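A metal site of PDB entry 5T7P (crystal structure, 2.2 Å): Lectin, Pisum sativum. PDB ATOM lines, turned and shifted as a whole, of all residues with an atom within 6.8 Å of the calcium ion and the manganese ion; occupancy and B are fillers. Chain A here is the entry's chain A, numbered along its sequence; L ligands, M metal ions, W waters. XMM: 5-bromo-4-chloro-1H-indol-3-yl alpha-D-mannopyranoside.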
ATOM      1  N   ASP A  81     -23.570 -21.002 -17.389  1.00  0.00           N
ATOM      2  CA  ASP A  81     -24.159 -20.549 -18.603  1.00  0.00           C
ATOM      3  C   ASP A  81     -24.452 -19.071 -18.495  1.00  0.00           C
ATOM      4  O   ASP A  81     -24.663 -18.429 -19.459  1.00  0.00           O
ATOM      5  CB  ASP A  81     -25.470 -21.230 -18.879  1.00  0.00           C
ATOM      6  CG  ASP A  81     -25.317 -22.476 -19.627  1.00  0.00           C
ATOM      7  OD1 ASP A  81     -25.166 -22.397 -20.789  1.00  0.00           O
ATOM      8  OD2 ASP A  81     -25.330 -23.542 -19.027  1.00  0.00           O
ATOM      9  N   GLY A  98     -29.597 -24.889 -18.521  1.00  0.00           N
ATOM     10  CA  GLY A  98     -28.512 -24.727 -19.479  1.00  0.00           C
ATOM     11  C   GLY A  98     -28.562 -23.355 -20.125  1.00  0.00           C
ATOM     12  O   GLY A  98     -28.790 -22.336 -19.456  1.00  0.00           O
ATOM     13  N   GLY A  99     -28.378 -23.314 -21.438  1.00  0.00           N
ATOM     14  CA  GLY A  99     -28.367 -22.058 -22.172  1.00  0.00           C
ATOM     15  C   GLY A  99     -29.680 -21.277 -22.108  1.00  0.00           C
ATOM     16  O   GLY A  99     -29.708 -20.114 -22.520  1.00  0.00           O
ATOM     17  N   TYR A 100     -30.749 -21.894 -21.612  1.00  0.00           N
ATOM     18  CA  TYR A 100     -32.019 -21.185 -21.467  1.00  0.00           C
ATOM     19  C   TYR A 100     -32.108 -20.368 -20.191  1.00  0.00           C
ATOM     20  O   TYR A 100     -33.099 -19.658 -20.006  1.00  0.00           O
ATOM     21  CB  TYR A 100     -33.181 -22.187 -21.550  1.00  0.00           C
ATOM     22  CG  TYR A 100     -33.365 -22.747 -22.934  1.00  0.00           C
ATOM     23  CD1 TYR A 100     -32.680 -23.892 -23.336  1.00  0.00           C
ATOM     24  CD2 TYR A 100     -34.198 -22.094 -23.862  1.00  0.00           C
ATOM     25  CE1 TYR A 100     -32.828 -24.391 -24.627  1.00  0.00           C
ATOM     26  CE2 TYR A 100     -34.351 -22.580 -25.134  1.00  0.00           C
ATOM     27  CZ  TYR A 100     -33.667 -23.733 -25.515  1.00  0.00           C
ATOM     28  OH  TYR A 100     -33.820 -24.218 -26.787  1.00  0.00           O
ATOM     29  N   LEU A 101     -31.114 -20.475 -19.313  1.00  0.00           N
ATOM     30  CA  LEU A 101     -30.957 -19.608 -18.149  1.00  0.00           C
ATOM     31  C   LEU A 101     -32.151 -19.688 -17.190  1.00  0.00           C
ATOM     32  O   LEU A 101     -32.385 -18.761 -16.403  1.00  0.00           O
ATOM     33  CB  LEU A 101     -30.706 -18.140 -18.574  1.00  0.00           C
ATOM     34  CG  LEU A 101     -29.467 -17.886 -19.449  1.00  0.00           C
ATOM     35  CD1 LEU A 101     -29.454 -16.491 -20.061  1.00  0.00           C
ATOM     36  CD2 LEU A 101     -28.173 -18.090 -18.687  1.00  0.00           C
ATOM     37  N   GLU A 119     -29.802 -10.600 -19.587  1.00  0.00           N
ATOM     38  CA  GLU A 119     -28.936 -11.758 -19.460  1.00  0.00           C
ATOM     39  C   GLU A 119     -27.482 -11.318 -19.500  1.00  0.00           C
ATOM     40  O   GLU A 119     -27.116 -10.354 -20.189  1.00  0.00           O
ATOM     41  CB  GLU A 119     -29.209 -12.812 -20.551  1.00  0.00           C
ATOM     42  CG  GLU A 119     -29.102 -12.342 -22.010  1.00  0.00           C
ATOM     43  CD  GLU A 119     -29.000 -13.488 -23.012  1.00  0.00           C
ATOM     44  OE1 GLU A 119     -28.024 -13.536 -23.786  1.00  0.00           O
ATOM     45  OE2 GLU A 119     -29.887 -14.357 -23.025  1.00  0.00           O
ATOM     46  N   ASP A 121     -24.588 -13.506 -20.377  1.00  0.00           N
ATOM     47  CA  ASP A 121     -24.576 -14.837 -20.987  1.00  0.00           C
ATOM     48  C   ASP A 121     -23.134 -15.220 -21.309  1.00  0.00           C
ATOM     49  O   ASP A 121     -22.516 -14.621 -22.202  1.00  0.00           O
ATOM     50  CB  ASP A 121     -25.452 -14.820 -22.249  1.00  0.00           C
ATOM     51  CG  ASP A 121     -25.531 -16.160 -22.943  1.00  0.00           C
ATOM     52  OD1 ASP A 121     -24.737 -17.072 -22.636  1.00  0.00           O
ATOM     53  OD2 ASP A 121     -26.379 -16.296 -23.824  1.00  0.00           O
ATOM     54  N   THR A 122     -22.612 -16.232 -20.613  1.00  0.00           N
ATOM     55  CA  THR A 122     -21.198 -16.581 -20.685  1.00  0.00           C
ATOM     56  C   THR A 122     -20.896 -17.709 -21.653  1.00  0.00           C
ATOM     57  O   THR A 122     -19.718 -18.048 -21.828  1.00  0.00           O
ATOM     58  CB  THR A 122     -20.669 -16.954 -19.311  1.00  0.00           C
ATOM     59  OG1 THR A 122     -21.429 -18.049 -18.774  1.00  0.00           O
ATOM     60  CG2 THR A 122     -20.753 -15.778 -18.372  1.00  0.00           C
ATOM     61  N   PHE A 123     -21.896 -18.301 -22.290  1.00  0.00           N
ATOM     62  CA  PHE A 123     -21.690 -19.478 -23.127  1.00  0.00           C
ATOM     63  C   PHE A 123     -22.419 -19.339 -24.459  1.00  0.00           C
ATOM     64  O   PHE A 123     -23.625 -19.107 -24.496  1.00  0.00           O
ATOM     65  CB  PHE A 123     -22.167 -20.754 -22.428  1.00  0.00           C
ATOM     66  CG  PHE A 123     -21.857 -22.004 -23.197  1.00  0.00           C
ATOM     67  CD1 PHE A 123     -20.623 -22.643 -23.074  1.00  0.00           C
ATOM     68  CD2 PHE A 123     -22.800 -22.554 -24.072  1.00  0.00           C
ATOM     69  CE1 PHE A 123     -20.342 -23.804 -23.797  1.00  0.00           C
ATOM     70  CE2 PHE A 123     -22.520 -23.716 -24.805  1.00  0.00           C
ATOM     71  CZ  PHE A 123     -21.300 -24.337 -24.662  1.00  0.00           C
ATOM     72  N   TYR A 124     -21.689 -19.554 -25.544  1.00  0.00           N
ATOM     73  CA  TYR A 124     -22.219 -19.423 -26.891  1.00  0.00           C
ATOM     74  C   TYR A 124     -23.094 -20.626 -27.223  1.00  0.00           C
ATOM     75  O   TYR A 124     -22.598 -21.730 -27.453  1.00  0.00           O
ATOM     76  CB  TYR A 124     -21.081 -19.285 -27.891  1.00  0.00           C
ATOM     77  CG  TYR A 124     -21.538 -19.381 -29.338  1.00  0.00           C
ATOM     78  CD1 TYR A 124     -22.273 -18.355 -29.908  1.00  0.00           C
ATOM     79  CD2 TYR A 124     -21.226 -20.506 -30.126  1.00  0.00           C
ATOM     80  CE1 TYR A 124     -22.703 -18.426 -31.218  1.00  0.00           C
ATOM     81  CE2 TYR A 124     -21.650 -20.582 -31.466  1.00  0.00           C
ATOM     82  CZ  TYR A 124     -22.390 -19.519 -31.999  1.00  0.00           C
ATOM     83  OH  TYR A 124     -22.829 -19.554 -33.300  1.00  0.00           O
ATOM     84  N   ASN A 125     -24.404 -20.421 -27.260  1.00  0.00           N
ATOM     85  CA  ASN A 125     -25.317 -21.437 -27.783  1.00  0.00           C
ATOM     86  C   ASN A 125     -25.539 -21.140 -29.255  1.00  0.00           C
ATOM     87  O   ASN A 125     -26.146 -20.117 -29.603  1.00  0.00           O
ATOM     88  CB  ASN A 125     -26.624 -21.452 -27.000  1.00  0.00           C
ATOM     89  CG  ASN A 125     -26.414 -21.810 -25.543  1.00  0.00           C
ATOM     90  OD1 ASN A 125     -26.259 -20.931 -24.702  1.00  0.00           O
ATOM     91  ND2 ASN A 125     -26.348 -23.116 -25.254  1.00  0.00           N
ATOM     92  N   TRP A 128     -28.855 -19.745 -31.155  1.00  0.00           N
ATOM     93  CA  TRP A 128     -29.468 -18.418 -31.032  1.00  0.00           C
ATOM     94  C   TRP A 128     -28.520 -17.281 -30.671  1.00  0.00           C
ATOM     95  O   TRP A 128     -28.879 -16.119 -30.888  1.00  0.00           O
ATOM     96  CB  TRP A 128     -30.572 -18.437 -29.993  1.00  0.00           C
ATOM     97  CG  TRP A 128     -30.131 -18.908 -28.636  1.00  0.00           C
ATOM     98  CD1 TRP A 128     -29.449 -18.206 -27.701  1.00  0.00           C
ATOM     99  CD2 TRP A 128     -30.367 -20.207 -28.064  1.00  0.00           C
ATOM    100  NE1 TRP A 128     -29.233 -18.973 -26.577  1.00  0.00           N
ATOM    101  CE2 TRP A 128     -29.793 -20.210 -26.769  1.00  0.00           C
ATOM    102  CE3 TRP A 128     -30.998 -21.369 -28.507  1.00  0.00           C
ATOM    103  CZ2 TRP A 128     -29.831 -21.319 -25.934  1.00  0.00           C
ATOM    104  CZ3 TRP A 128     -31.040 -22.488 -27.671  1.00  0.00           C
ATOM    105  CH2 TRP A 128     -30.473 -22.447 -26.399  1.00  0.00           C
ATOM    106  N   ASP A 129     -27.363 -17.579 -30.074  1.00  0.00           N
ATOM    107  CA  ASP A 129     -26.518 -16.516 -29.539  1.00  0.00           C
ATOM    108  C   ASP A 129     -25.808 -15.747 -30.652  1.00  0.00           C
ATOM    109  O   ASP A 129     -25.673 -16.254 -31.762  1.00  0.00           O
ATOM    110  CB  ASP A 129     -25.517 -17.094 -28.548  1.00  0.00           C
ATOM    111  CG  ASP A 129     -26.058 -17.106 -27.139  1.00  0.00           C
ATOM    112  OD1 ASP A 129     -26.986 -16.316 -26.894  1.00  0.00           O
ATOM    113  OD2 ASP A 129     -25.580 -17.906 -26.284  1.00  0.00           O
ATOM    114  N   PRO A 130     -25.346 -14.530 -30.371  1.00  0.00           N
ATOM    115  CA  PRO A 130     -24.694 -13.724 -31.422  1.00  0.00           C
ATOM    116  C   PRO A 130     -23.540 -14.481 -32.048  1.00  0.00           C
ATOM    117  O   PRO A 130     -22.777 -15.176 -31.372  1.00  0.00           O
ATOM    118  CB  PRO A 130     -24.219 -12.476 -30.671  1.00  0.00           C
ATOM    119  CG  PRO A 130     -25.169 -12.348 -29.523  1.00  0.00           C
ATOM    120  CD  PRO A 130     -25.460 -13.780 -29.098  1.00  0.00           C
ATOM    121  N   HIS A 136     -21.852 -12.000 -23.725  1.00  0.00           N
ATOM    122  CA  HIS A 136     -22.658 -10.846 -24.108  1.00  0.00           C
ATOM    123  C   HIS A 136     -23.717 -10.561 -23.073  1.00  0.00           C
ATOM    124  O   HIS A 136     -24.266 -11.466 -22.435  1.00  0.00           O
ATOM    125  CB  HIS A 136     -23.321 -11.052 -25.471  1.00  0.00           C
ATOM    126  CG  HIS A 136     -24.118 -12.312 -25.553  1.00  0.00           C
ATOM    127  ND1 HIS A 136     -23.539 -13.534 -25.822  1.00  0.00           N
ATOM    128  CD2 HIS A 136     -25.442 -12.552 -25.396  1.00  0.00           C
ATOM    129  CE1 HIS A 136     -24.480 -14.460 -25.846  1.00  0.00           C
ATOM    130  NE2 HIS A 136     -25.633 -13.888 -25.589  1.00  0.00           N
ATOM    131  N   ILE A 137     -24.006  -9.283 -22.921  1.00  0.00           N
ATOM    132  CA  ILE A 137     -25.187  -8.818 -22.232  1.00  0.00           C
ATOM    133  C   ILE A 137     -26.324  -8.853 -23.230  1.00  0.00           C
ATOM    134  O   ILE A 137     -26.123  -8.603 -24.418  1.00  0.00           O
ATOM    135  CB  ILE A 137     -24.947  -7.399 -21.666  1.00  0.00           C
ATOM    136  CG1 ILE A 137     -23.815  -7.443 -20.622  1.00  0.00           C
ATOM    137  CG2 ILE A 137     -26.213  -6.829 -21.079  1.00  0.00           C
ATOM    138  CD1 ILE A 137     -23.102  -6.102 -20.449  1.00  0.00           C
ATOM    139  N   GLY A 138     -27.518  -9.218 -22.782  1.00  0.00           N
ATOM    140  CA  GLY A 138     -28.651  -9.287 -23.678  1.00  0.00           C
ATOM    141  C   GLY A 138     -29.912  -8.806 -23.004  1.00  0.00           C
ATOM    142  O   GLY A 138     -30.043  -8.864 -21.783  1.00  0.00           O
ATOM    143  N   ASP A 140     -33.811  -9.848 -23.281  1.00  0.00           N
ATOM    144  CA  ASP A 140     -34.566 -10.992 -23.776  1.00  0.00           C
ATOM    145  C   ASP A 140     -36.043 -10.724 -23.554  1.00  0.00           C
ATOM    146  O   ASP A 140     -36.454 -10.363 -22.442  1.00  0.00           O
ATOM    147  CB  ASP A 140     -34.190 -12.268 -23.041  1.00  0.00           C
ATOM    148  CG  ASP A 140     -32.730 -12.628 -23.165  1.00  0.00           C
ATOM    149  OD1 ASP A 140     -31.999 -12.019 -23.997  1.00  0.00           O
ATOM    150  OD2 ASP A 140     -32.331 -13.572 -22.444  1.00  0.00           O
ATOM    151  N   ILE A 144     -35.109 -16.752 -25.600  1.00  0.00           N
ATOM    152  CA  ILE A 144     -33.695 -16.803 -25.240  1.00  0.00           C
ATOM    153  C   ILE A 144     -32.827 -16.137 -26.297  1.00  0.00           C
ATOM    154  O   ILE A 144     -31.628 -15.935 -26.090  1.00  0.00           O
ATOM    155  CB  ILE A 144     -33.237 -18.253 -25.011  1.00  0.00           C
ATOM    156  CG1 ILE A 144     -31.943 -18.322 -24.178  1.00  0.00           C
ATOM    157  CG2 ILE A 144     -33.038 -18.966 -26.353  1.00  0.00           C
ATOM    158  CD1 ILE A 144     -31.950 -17.449 -22.902  1.00  0.00           C
ATOM    159  N   LYS A 145     -33.413 -15.774 -27.435  1.00  0.00           N
ATOM    160  CA  LYS A 145     -32.715 -15.048 -28.484  1.00  0.00           C
ATOM    161  C   LYS A 145     -32.956 -13.563 -28.229  1.00  0.00           C
ATOM    162  O   LYS A 145     -34.065 -13.065 -28.462  1.00  0.00           O
ATOM    163  CB  LYS A 145     -33.216 -15.484 -29.863  1.00  0.00           C
ATOM    164  CG  LYS A 145     -32.448 -14.901 -31.038  1.00  0.00           C
ATOM    165  CD  LYS A 145     -33.091 -15.354 -32.345  1.00  0.00           C
ATOM    166  CE  LYS A 145     -32.267 -14.966 -33.560  1.00  0.00           C
ATOM    167  NZ  LYS A 145     -32.296 -16.058 -34.596  1.00  0.00           N
ATOM    168  N   SER A 146     -31.939 -12.873 -27.731  1.00  0.00           N
ATOM    169  CA  SER A 146     -32.096 -11.507 -27.293  1.00  0.00           C
ATOM    170  C   SER A 146     -32.518 -10.597 -28.452  1.00  0.00           C
ATOM    171  O   SER A 146     -32.033 -10.750 -29.573  1.00  0.00           O
ATOM    172  CB  SER A 146     -30.784 -10.987 -26.694  1.00  0.00           C
ATOM    173  OG  SER A 146     -30.229 -11.912 -25.746  1.00  0.00           O
ATOM    174  N   THR A 149     -28.087  -7.198 -28.080  1.00  0.00           N
ATOM    175  CA  THR A 149     -26.961  -7.749 -27.341  1.00  0.00           C
ATOM    176  C   THR A 149     -25.770  -6.818 -27.446  1.00  0.00           C
ATOM    177  O   THR A 149     -25.652  -6.035 -28.385  1.00  0.00           O
ATOM    178  CB  THR A 149     -26.540  -9.141 -27.848  1.00  0.00           C
ATOM    179  OG1 THR A 149     -26.195  -9.057 -29.227  1.00  0.00           O
ATOM    180  CG2 THR A 149     -27.640 -10.159 -27.643  1.00  0.00           C
HETATM  181  O2  XMM L   1     -26.911 -27.781 -21.484  1.00  0.00           O
HETATM  182  C2  XMM L   1     -26.247 -27.595 -22.733  1.00  0.00           C
HETATM  183  C3  XMM L   1     -26.384 -26.139 -23.168  1.00  0.00           C
HETATM  184  O3  XMM L   1     -27.757 -25.739 -23.073  1.00  0.00           O
HETATM  185  C4  XMM L   1     -25.522 -25.221 -22.312  1.00  0.00           C
HETATM  186  O4  XMM L   1     -25.495 -23.912 -22.879  1.00  0.00           O
HETATM  187  C5  XMM L   1     -24.093 -25.760 -22.200  1.00  0.00           C
HETATM  188  O5  XMM L   1     -24.123 -27.096 -21.701  1.00  0.00           O
HETATM  189  C6  XMM L   1     -23.256 -24.891 -21.279  1.00  0.00           C
HETATM  190  O6  XMM L   1     -23.406 -25.345 -19.929  1.00  0.00           O
HETATM  191  C1  XMM L   1     -24.775 -27.987 -22.605  1.00  0.00           C
HETATM  192  O1  XMM L   1     -24.144 -27.919 -23.873  1.00  0.00           O
HETATM  193  C7  XMM L   1     -22.960 -28.562 -24.088  1.00  0.00           C
HETATM  194  C8  XMM L   1     -22.840 -29.988 -24.408  1.00  0.00           C
HETATM  195  C9  XMM L   1     -21.364 -30.129 -24.529  1.00  0.00           C
HETATM  196  N1  XMM L   1     -20.802 -28.921 -24.305  1.00  0.00           N
HETATM  197  C11 XMM L   1     -21.723 -27.940 -24.034  1.00  0.00           C
HETATM  198  C10 XMM L   1     -23.716 -31.156 -24.601  1.00  0.00           C
HETATM  199 CL   XMM L   1     -25.504 -31.031 -24.466  1.00  0.00          CL
HETATM  200  C13 XMM L   1     -23.056 -32.444 -24.921  1.00  0.00           C
HETATM  201 BR   XMM L   1     -24.090 -34.011 -25.195  1.00  0.00          BR
HETATM  202  C14 XMM L   1     -21.666 -32.499 -25.022  1.00  0.00           C
HETATM  203  C12 XMM L   1     -20.842 -31.388 -24.831  1.00  0.00           C
HETATM  204 CA    CA M   1     -25.810 -18.668 -24.112  1.00  0.00          CA
HETATM  205 MN    MN M   2     -27.416 -15.052 -25.212  1.00  0.00          MN
HETATM  206  O   HOH W   1     -28.608 -13.727 -26.674  1.00  0.00           O
HETATM  207  O   HOH W   2     -29.412 -16.068 -24.638  1.00  0.00           O
HETATM  208  O   HOH W   3     -28.180 -18.524 -24.044  1.00  0.00           O
HETATM  209  O   HOH W   4     -25.537 -19.747 -21.954  1.00  0.00           O
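O4 of the ligand sits at hydrogen-bond distance from ND2 of Asn 125. An oxygen (O4) of the ligand sits at hydrogen-bond distance from the side-chain carboxylate of Asp 81 (2.6 Å). The backbone NH (N) of Gly 99 sits at hydrogen-bond distance from an oxygen (O3) of the ligand (3.0 Å).
OE1 of Glu 119 sits close to OG of Ser 146, at 3.4 Å. The side-chain carboxylate of Asp 140 lies close to the side-chain carboxylate of Glu 119 (2.6 Å). The side-chain carboxylate of Asp 129 lies close to the indole nitrogen of Trp 128, 3.5 Å away. The backbone NH (N) of Glu 119 lies within hydrogen-bond range of the backbone carbonyl oxygen (O) of Gly 138 (2.8 Å).
The calcium ion is bound by O of Phe 123, at 2.3 Å. OD2 of Asp 129 binds the calcium ion, 2.3 Å away. The calcium ion is bound by water W3. OD1 of Asn 125 is bound to the calcium ion, at 2.4 Å. OD1 of Asp 121 binds the calcium ion (2.4 Å). Water W4 binds the calcium ion. The side-chain carboxylate (OD2) of Asp 121 binds the calcium ion (2.5 Å). The calcium ion has seven donor atoms within binding distance.
Within 4 Å of the manganese ion: Glu 119, Asp 121, Asp 129 and His 136. The nearest printed residue that does not touch the manganese ion is Ser 146 (4.2 Å).
The manganese ion is bound by OD2 of Asp 121 (2.1 Å), OD1 of Asp 129 (2.1 Å), NE2 of His 136 (2.2 Å), OE1 of Glu 119 (2.2 Å), water W1 (2.3 Å) and water W2 (2.3 Å).
Water W3 bridges the backbone carbonyl oxygen (O) of Gly 99 (2.7 Å) and the indole nitrogen (NE1) of Trp 128 (2.8 Å). Water W2 lies within hydrogen-bond range of the backbone carbonyl oxygen (O) of Ile 144 (2.7 Å) and the indole nitrogen (NE1) of Trp 128 (3.5 Å).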
